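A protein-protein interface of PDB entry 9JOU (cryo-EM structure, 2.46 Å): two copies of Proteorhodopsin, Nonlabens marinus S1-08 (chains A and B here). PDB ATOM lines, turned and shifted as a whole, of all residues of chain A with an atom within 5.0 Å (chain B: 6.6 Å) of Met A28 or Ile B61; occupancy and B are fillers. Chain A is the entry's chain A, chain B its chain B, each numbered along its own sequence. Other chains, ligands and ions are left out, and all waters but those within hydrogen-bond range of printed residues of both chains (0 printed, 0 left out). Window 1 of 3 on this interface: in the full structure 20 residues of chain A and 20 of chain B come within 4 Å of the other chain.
Among the printed residues, merely in contact across the chains: Phe A24 with Val B86, Val A25 with Leu B90, Met A28 with Ile B61, Met A28 with Val B64, Ala A29 with Leu B90, Met A31 with Phe B60, Met A31 with Val B64, Ala A32 with Leu B57 and Ala A32 with Ile B61.
Printed residues of chain B within 4 Å of Met A28: Ile B61 and Val B64.
Ile B61 touches just these residues of chain A: Met A28 and Ala A32.
Of the printed residues of chain B, Val A25 touches Leu B90 (3.5 Å).
Of the printed residues of chain A, Leu B57 touches Ala A32 (3.5 Å).
Printed residues of chain A within 4 Å of Leu B90: Val A25 and Ala A29.
Printed residues of chain A within 4 Å of Val B86: Phe A24 (3.99 Å).
The nearest printed residue of chain A that does not touch Ile B61 is Met A31 (5.1 Å).
The nearest printed residue of chain A that does not touch Val B86 is Met A28 (4.2 Å).
Hydrophobic or aromatic side chains of chain B that line the printed part of chain A: Leu B57, Phe B60, Ile B61, Val B64, Val B86 and Leu B90.
Of the 10 printed residues of chain A, 6 touch a printed residue of chain B.
Printed residues of chain A that touch a printed residue of chain B: Phe A24, Val A25, Met A28, Ala A29, Met A31 and Ala A32.
Hydrophobic or aromatic side chains of chain A that line the printed part of chain B: Phe A24, Val A25, Met A28, Ala A29, Met A31 and Ala A32.
Among the printed residues, no Asp or Glu carboxylate lies within 4 Å of a Lys or Arg side-chain nitrogen of the other chain.
Position printed for both chains: 30.
Of the 9 pairs that touch across the chains among the printed residues, none has its exchanged pair printed and touching as well.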
ATOM      1  N   PHE A  23       6.943 -12.865   8.901  1.00  0.00           N
ATOM      2  CA  PHE A  23       6.648 -12.975  10.327  1.00  0.00           C
ATOM      3  C   PHE A  23       7.662 -13.884  11.013  1.00  0.00           C
ATOM      4  O   PHE A  23       8.261 -13.496  12.025  1.00  0.00           O
ATOM      5  CB  PHE A  23       5.249 -13.508  10.606  1.00  0.00           C
ATOM      6  CG  PHE A  23       4.204 -12.412  10.626  1.00  0.00           C
ATOM      7  CD1 PHE A  23       4.445 -11.241  11.334  1.00  0.00           C
ATOM      8  CD2 PHE A  23       3.016 -12.542   9.912  1.00  0.00           C
ATOM      9  CE1 PHE A  23       3.485 -10.234  11.358  1.00  0.00           C
ATOM     10  CE2 PHE A  23       2.073 -11.521   9.915  1.00  0.00           C
ATOM     11  CZ  PHE A  23       2.306 -10.375  10.639  1.00  0.00           C
ATOM     12  N   PHE A  24       7.891 -15.071  10.435  1.00  0.00           N
ATOM     13  CA  PHE A  24       8.802 -16.036  11.039  1.00  0.00           C
ATOM     14  C   PHE A  24      10.224 -15.491  11.109  1.00  0.00           C
ATOM     15  O   PHE A  24      10.946 -15.731  12.061  1.00  0.00           O
ATOM     16  CB  PHE A  24       8.809 -17.336  10.251  1.00  0.00           C
ATOM     17  CG  PHE A  24       7.751 -18.322  10.703  1.00  0.00           C
ATOM     18  CD1 PHE A  24       6.471 -18.265  10.183  1.00  0.00           C
ATOM     19  CD2 PHE A  24       8.049 -19.307  11.647  1.00  0.00           C
ATOM     20  CE1 PHE A  24       5.510 -19.180  10.576  1.00  0.00           C
ATOM     21  CE2 PHE A  24       7.085 -20.215  12.039  1.00  0.00           C
ATOM     22  CZ  PHE A  24       5.816 -20.149  11.504  1.00  0.00           C
ATOM     23  N   VAL A  25      10.643 -14.758  10.085  1.00  0.00           N
ATOM     24  CA  VAL A  25      11.999 -14.238  10.079  1.00  0.00           C
ATOM     25  C   VAL A  25      12.097 -13.161  11.146  1.00  0.00           C
ATOM     26  O   VAL A  25      13.067 -13.146  11.905  1.00  0.00           O
ATOM     27  CB  VAL A  25      12.398 -13.704   8.694  1.00  0.00           C
ATOM     28  CG1 VAL A  25      13.784 -13.096   8.718  1.00  0.00           C
ATOM     29  CG2 VAL A  25      12.361 -14.806   7.676  1.00  0.00           C
ATOM     30  N   GLY A  26      11.116 -12.238  11.132  1.00  0.00           N
ATOM     31  CA  GLY A  26      11.092 -11.116  12.055  1.00  0.00           C
ATOM     32  C   GLY A  26      11.083 -11.620  13.498  1.00  0.00           C
ATOM     33  O   GLY A  26      11.941 -11.279  14.328  1.00  0.00           O
ATOM     34  N   CYS A  27      10.157 -12.526  13.776  1.00  0.00           N
ATOM     35  CA  CYS A  27      10.110 -13.092  15.115  1.00  0.00           C
ATOM     36  C   CYS A  27      11.452 -13.680  15.539  1.00  0.00           C
ATOM     37  O   CYS A  27      11.851 -13.449  16.682  1.00  0.00           O
ATOM     38  CB  CYS A  27       9.086 -14.199  15.258  1.00  0.00           C
ATOM     39  SG  CYS A  27       9.109 -14.829  16.953  1.00  0.00           S
ATOM     40  N   MET A  28      12.116 -14.442  14.634  1.00  0.00           N
ATOM     41  CA  MET A  28      13.374 -15.118  14.943  1.00  0.00           C
ATOM     42  C   MET A  28      14.513 -14.119  15.127  1.00  0.00           C
ATOM     43  O   MET A  28      15.301 -14.254  16.078  1.00  0.00           O
ATOM     44  CB  MET A  28      13.783 -16.123  13.869  1.00  0.00           C
ATOM     45  CG  MET A  28      12.887 -17.340  13.776  1.00  0.00           C
ATOM     46  SD  MET A  28      12.913 -18.457  15.198  1.00  0.00           S
ATOM     47  CE  MET A  28      14.400 -18.102  16.137  1.00  0.00           C
ATOM     48  N   ALA A  29      14.570 -13.116  14.227  1.00  0.00           N
ATOM     49  CA  ALA A  29      15.617 -12.101  14.272  1.00  0.00           C
ATOM     50  C   ALA A  29      15.469 -11.228  15.524  1.00  0.00           C
ATOM     51  O   ALA A  29      16.456 -10.808  16.124  1.00  0.00           O
ATOM     52  CB  ALA A  29      15.575 -11.268  13.014  1.00  0.00           C
ATOM     53  N   MET A  30      14.229 -10.933  15.921  1.00  0.00           N
ATOM     54  CA  MET A  30      14.036 -10.127  17.118  1.00  0.00           C
ATOM     55  C   MET A  30      14.459 -10.941  18.347  1.00  0.00           C
ATOM     56  O   MET A  30      15.256 -10.493  19.183  1.00  0.00           O
ATOM     57  CB  MET A  30      12.574  -9.678  17.218  1.00  0.00           C
ATOM     58  CG  MET A  30      12.377  -8.218  17.502  1.00  0.00           C
ATOM     59  SD  MET A  30      12.386  -7.187  16.020  1.00  0.00           S
ATOM     60  CE  MET A  30      10.815  -7.610  15.257  1.00  0.00           C
ATOM     61  N   MET A  31      14.031 -12.201  18.415  1.00  0.00           N
ATOM     62  CA  MET A  31      14.440 -13.055  19.527  1.00  0.00           C
ATOM     63  C   MET A  31      15.958 -13.166  19.643  1.00  0.00           C
ATOM     64  O   MET A  31      16.481 -13.187  20.766  1.00  0.00           O
ATOM     65  CB  MET A  31      13.901 -14.470  19.366  1.00  0.00           C
ATOM     66  CG  MET A  31      14.299 -15.427  20.467  1.00  0.00           C
ATOM     67  SD  MET A  31      13.800 -17.088  19.981  1.00  0.00           S
ATOM     68  CE  MET A  31      12.202 -16.708  19.237  1.00  0.00           C
ATOM     69  N   ALA A  32      16.655 -13.249  18.495  1.00  0.00           N
ATOM     70  CA  ALA A  32      18.109 -13.363  18.496  1.00  0.00           C
ATOM     71  C   ALA A  32      18.765 -12.094  19.011  1.00  0.00           C
ATOM     72  O   ALA A  32      19.542 -12.139  19.973  1.00  0.00           O
ATOM     73  CB  ALA A  32      18.591 -13.675  17.091  1.00  0.00           C
ATOM     74  N   MET B  30      20.990 -28.906  19.381  1.00  0.00           N
ATOM     75  CA  MET B  30      21.147 -27.474  19.195  1.00  0.00           C
ATOM     76  C   MET B  30      20.808 -26.750  20.513  1.00  0.00           C
ATOM     77  O   MET B  30      21.582 -25.931  21.019  1.00  0.00           O
ATOM     78  CB  MET B  30      20.245 -26.997  18.056  1.00  0.00           C
ATOM     79  CG  MET B  30      20.909 -26.110  17.046  1.00  0.00           C
ATOM     80  SD  MET B  30      21.834 -26.924  15.734  1.00  0.00           S
ATOM     81  CE  MET B  30      20.455 -27.638  14.818  1.00  0.00           C
ATOM     82  N   SER B  34      23.423 -24.432  22.434  1.00  0.00           N
ATOM     83  CA  SER B  34      23.107 -23.021  22.709  1.00  0.00           C
ATOM     84  C   SER B  34      23.347 -22.666  24.161  1.00  0.00           C
ATOM     85  O   SER B  34      23.959 -21.639  24.456  1.00  0.00           O
ATOM     86  CB  SER B  34      21.727 -22.632  22.323  1.00  0.00           C
ATOM     87  OG  SER B  34      20.851 -23.748  22.355  1.00  0.00           O
ATOM     88  N   GLY B  56      26.758 -19.212  19.949  1.00  0.00           N
ATOM     89  CA  GLY B  56      25.526 -19.559  20.629  1.00  0.00           C
ATOM     90  C   GLY B  56      24.279 -19.050  19.897  1.00  0.00           C
ATOM     91  O   GLY B  56      23.411 -19.865  19.529  1.00  0.00           O
ATOM     92  N   LEU B  57      24.178 -17.724  19.670  1.00  0.00           N
ATOM     93  CA  LEU B  57      23.044 -17.229  18.906  1.00  0.00           C
ATOM     94  C   LEU B  57      22.716 -18.119  17.718  1.00  0.00           C
ATOM     95  O   LEU B  57      21.544 -18.499  17.577  1.00  0.00           O
ATOM     96  CB  LEU B  57      23.181 -15.780  18.436  1.00  0.00           C
ATOM     97  CG  LEU B  57      22.816 -14.733  19.493  1.00  0.00           C
ATOM     98  CD1 LEU B  57      21.548 -15.029  20.236  1.00  0.00           C
ATOM     99  CD2 LEU B  57      23.901 -14.640  20.509  1.00  0.00           C
ATOM    100  N   ILE B  58      23.736 -18.432  16.870  1.00  0.00           N
ATOM    101  CA  ILE B  58      23.545 -19.341  15.747  1.00  0.00           C
ATOM    102  C   ILE B  58      22.871 -20.633  16.187  1.00  0.00           C
ATOM    103  O   ILE B  58      21.833 -20.992  15.610  1.00  0.00           O
ATOM    104  CB  ILE B  58      24.856 -19.673  14.983  1.00  0.00           C
ATOM    105  CG1 ILE B  58      25.471 -18.474  14.255  1.00  0.00           C
ATOM    106  CG2 ILE B  58      24.597 -20.767  13.946  1.00  0.00           C
ATOM    107  CD1 ILE B  58      26.951 -18.618  13.947  1.00  0.00           C
ATOM    108  N   THR B  59      23.450 -21.349  17.173  1.00  0.00           N
ATOM    109  CA  THR B  59      22.762 -22.562  17.597  1.00  0.00           C
ATOM    110  C   THR B  59      21.373 -22.207  18.119  1.00  0.00           C
ATOM    111  O   THR B  59      20.391 -22.926  17.849  1.00  0.00           O
ATOM    112  CB  THR B  59      23.527 -23.403  18.631  1.00  0.00           C
ATOM    113  OG1 THR B  59      23.828 -22.686  19.821  1.00  0.00           O
ATOM    114  CG2 THR B  59      24.821 -23.984  18.105  1.00  0.00           C
ATOM    115  N   PHE B  60      21.261 -21.080  18.840  1.00  0.00           N
ATOM    116  CA  PHE B  60      19.963 -20.745  19.429  1.00  0.00           C
ATOM    117  C   PHE B  60      18.870 -20.587  18.376  1.00  0.00           C
ATOM    118  O   PHE B  60      17.819 -21.203  18.488  1.00  0.00           O
ATOM    119  CB  PHE B  60      20.160 -19.507  20.303  1.00  0.00           C
ATOM    120  CG  PHE B  60      18.893 -19.066  21.002  1.00  0.00           C
ATOM    121  CD1 PHE B  60      18.023 -19.993  21.550  1.00  0.00           C
ATOM    122  CD2 PHE B  60      18.550 -17.718  21.055  1.00  0.00           C
ATOM    123  CE1 PHE B  60      16.840 -19.584  22.137  1.00  0.00           C
ATOM    124  CE2 PHE B  60      17.378 -17.311  21.678  1.00  0.00           C
ATOM    125  CZ  PHE B  60      16.522 -18.250  22.203  1.00  0.00           C
ATOM    126  N   ILE B  61      19.134 -19.781  17.324  1.00  0.00           N
ATOM    127  CA  ILE B  61      18.135 -19.606  16.288  1.00  0.00           C
ATOM    128  C   ILE B  61      17.751 -20.954  15.702  1.00  0.00           C
ATOM    129  O   ILE B  61      16.575 -21.247  15.552  1.00  0.00           O
ATOM    130  CB  ILE B  61      18.609 -18.621  15.196  1.00  0.00           C
ATOM    131  CG1 ILE B  61      18.849 -17.236  15.736  1.00  0.00           C
ATOM    132  CG2 ILE B  61      17.616 -18.560  14.054  1.00  0.00           C
ATOM    133  CD1 ILE B  61      18.005 -16.948  16.963  1.00  0.00           C
ATOM    134  N   ALA B  62      18.749 -21.758  15.303  1.00  0.00           N
ATOM    135  CA  ALA B  62      18.524 -23.133  14.851  1.00  0.00           C
ATOM    136  C   ALA B  62      17.694 -23.942  15.861  1.00  0.00           C
ATOM    137  O   ALA B  62      16.633 -24.476  15.509  1.00  0.00           O
ATOM    138  CB  ALA B  62      19.865 -23.791  14.599  1.00  0.00           C
ATOM    139  N   ALA B  63      18.112 -24.035  17.137  1.00  0.00           N
ATOM    140  CA  ALA B  63      17.266 -24.779  18.093  1.00  0.00           C
ATOM    141  C   ALA B  63      15.798 -24.382  18.023  1.00  0.00           C
ATOM    142  O   ALA B  63      14.928 -25.252  17.974  1.00  0.00           O
ATOM    143  CB  ALA B  63      17.703 -24.578  19.526  1.00  0.00           C
ATOM    144  N   VAL B  64      15.512 -23.060  18.030  1.00  0.00           N
ATOM    145  CA  VAL B  64      14.131 -22.599  18.030  1.00  0.00           C
ATOM    146  C   VAL B  64      13.436 -22.964  16.725  1.00  0.00           C
ATOM    147  O   VAL B  64      12.297 -23.429  16.769  1.00  0.00           O
ATOM    148  CB  VAL B  64      13.998 -21.102  18.374  1.00  0.00           C
ATOM    149  CG1 VAL B  64      12.594 -20.567  18.203  1.00  0.00           C
ATOM    150  CG2 VAL B  64      14.474 -20.816  19.797  1.00  0.00           C
ATOM    151  N   HIS B  65      14.119 -22.791  15.576  1.00  0.00           N
ATOM    152  CA  HIS B  65      13.498 -23.178  14.323  1.00  0.00           C
ATOM    153  C   HIS B  65      13.345 -24.696  14.280  1.00  0.00           C
ATOM    154  O   HIS B  65      12.286 -25.215  13.923  1.00  0.00           O
ATOM    155  CB  HIS B  65      14.194 -22.538  13.111  1.00  0.00           C
ATOM    156  CG  HIS B  65      13.328 -22.564  11.889  1.00  0.00           C
ATOM    157  ND1 HIS B  65      12.088 -21.970  11.848  1.00  0.00           N
ATOM    158  CD2 HIS B  65      13.501 -23.109  10.676  1.00  0.00           C
ATOM    159  CE1 HIS B  65      11.525 -22.186  10.659  1.00  0.00           C
ATOM    160  NE2 HIS B  65      12.380 -22.849   9.921  1.00  0.00           N
ATOM    161  N   TYR B  66      14.381 -25.441  14.680  1.00  0.00           N
ATOM    162  CA  TYR B  66      14.279 -26.897  14.640  1.00  0.00           C
ATOM    163  C   TYR B  66      13.080 -27.391  15.444  1.00  0.00           C
ATOM    164  O   TYR B  66      12.371 -28.288  14.982  1.00  0.00           O
ATOM    165  CB  TYR B  66      15.512 -27.662  15.126  1.00  0.00           C
ATOM    166  CG  TYR B  66      16.330 -28.146  13.939  1.00  0.00           C
ATOM    167  CD1 TYR B  66      16.841 -27.242  13.016  1.00  0.00           C
ATOM    168  CD2 TYR B  66      16.500 -29.502  13.678  1.00  0.00           C
ATOM    169  CE1 TYR B  66      17.542 -27.666  11.902  1.00  0.00           C
ATOM    170  CE2 TYR B  66      17.203 -29.939  12.571  1.00  0.00           C
ATOM    171  CZ  TYR B  66      17.719 -29.015  11.677  1.00  0.00           C
ATOM    172  OH  TYR B  66      18.423 -29.359  10.569  1.00  0.00           O
ATOM    173  N   VAL B  86      14.029 -19.723   6.506  1.00  0.00           N
ATOM    174  CA  VAL B  86      13.762 -18.965   7.727  1.00  0.00           C
ATOM    175  C   VAL B  86      14.988 -18.967   8.631  1.00  0.00           C
ATOM    176  O   VAL B  86      15.368 -17.934   9.177  1.00  0.00           O
ATOM    177  CB  VAL B  86      12.564 -19.517   8.515  1.00  0.00           C
ATOM    178  CG1 VAL B  86      12.473 -18.859   9.873  1.00  0.00           C
ATOM    179  CG2 VAL B  86      11.239 -19.373   7.770  1.00  0.00           C
ATOM    180  N   ASP B  87      15.587 -20.147   8.819  1.00  0.00           N
ATOM    181  CA  ASP B  87      16.778 -20.255   9.640  1.00  0.00           C
ATOM    182  C   ASP B  87      17.996 -19.769   8.860  1.00  0.00           C
ATOM    183  O   ASP B  87      18.717 -18.890   9.334  1.00  0.00           O
ATOM    184  CB  ASP B  87      16.930 -21.669  10.177  1.00  0.00           C
ATOM    185  CG  ASP B  87      18.220 -21.989  10.913  1.00  0.00           C
ATOM    186  OD1 ASP B  87      18.925 -21.039  11.313  1.00  0.00           O
ATOM    187  OD2 ASP B  87      18.521 -23.193  11.064  1.00  0.00           O
ATOM    188  N   LEU B  90      19.154 -16.186   8.403  1.00  0.00           N
ATOM    189  CA  LEU B  90      19.652 -15.566   9.626  1.00  0.00           C
ATOM    190  C   LEU B  90      21.051 -16.083   9.968  1.00  0.00           C
ATOM    191  O   LEU B  90      21.920 -15.322  10.382  1.00  0.00           O
ATOM    192  CB  LEU B  90      18.717 -15.775  10.826  1.00  0.00           C
ATOM    193  CG  LEU B  90      17.635 -14.727  11.096  1.00  0.00           C
ATOM    194  CD1 LEU B  90      18.233 -13.359  11.374  1.00  0.00           C
ATOM    195  CD2 LEU B  90      16.689 -14.648   9.928  1.00  0.00           C
ATOM    196  N   THR B  91      21.268 -17.397   9.846  1.00  0.00           N
ATOM    197  CA  THR B  91      22.438 -18.024  10.437  1.00  0.00           C
ATOM    198  C   THR B  91      23.645 -17.904   9.524  1.00  0.00           C
ATOM    199  O   THR B  91      24.727 -17.515   9.976  1.00  0.00           O
ATOM    200  CB  THR B  91      22.096 -19.469  10.776  1.00  0.00           C
ATOM    201  OG1 THR B  91      21.176 -19.792   9.734  1.00  0.00           O
ATOM    202  CG2 THR B  91      21.461 -19.601  12.158  1.00  0.00           C
ATOM    203  N   LEU B  94      25.676 -14.972  10.065  1.00  0.00           N
ATOM    204  CA  LEU B  94      26.382 -14.920  11.337  1.00  0.00           C
ATOM    205  C   LEU B  94      27.686 -15.703  11.231  1.00  0.00           C
ATOM    206  O   LEU B  94      28.747 -15.204  11.602  1.00  0.00           O
ATOM    207  CB  LEU B  94      25.530 -15.374  12.514  1.00  0.00           C
ATOM    208  CG  LEU B  94      24.247 -14.563  12.744  1.00  0.00           C
ATOM    209  CD1 LEU B  94      23.527 -15.033  13.978  1.00  0.00           C
ATOM    210  CD2 LEU B  94      24.482 -13.075  12.842  1.00  0.00           C
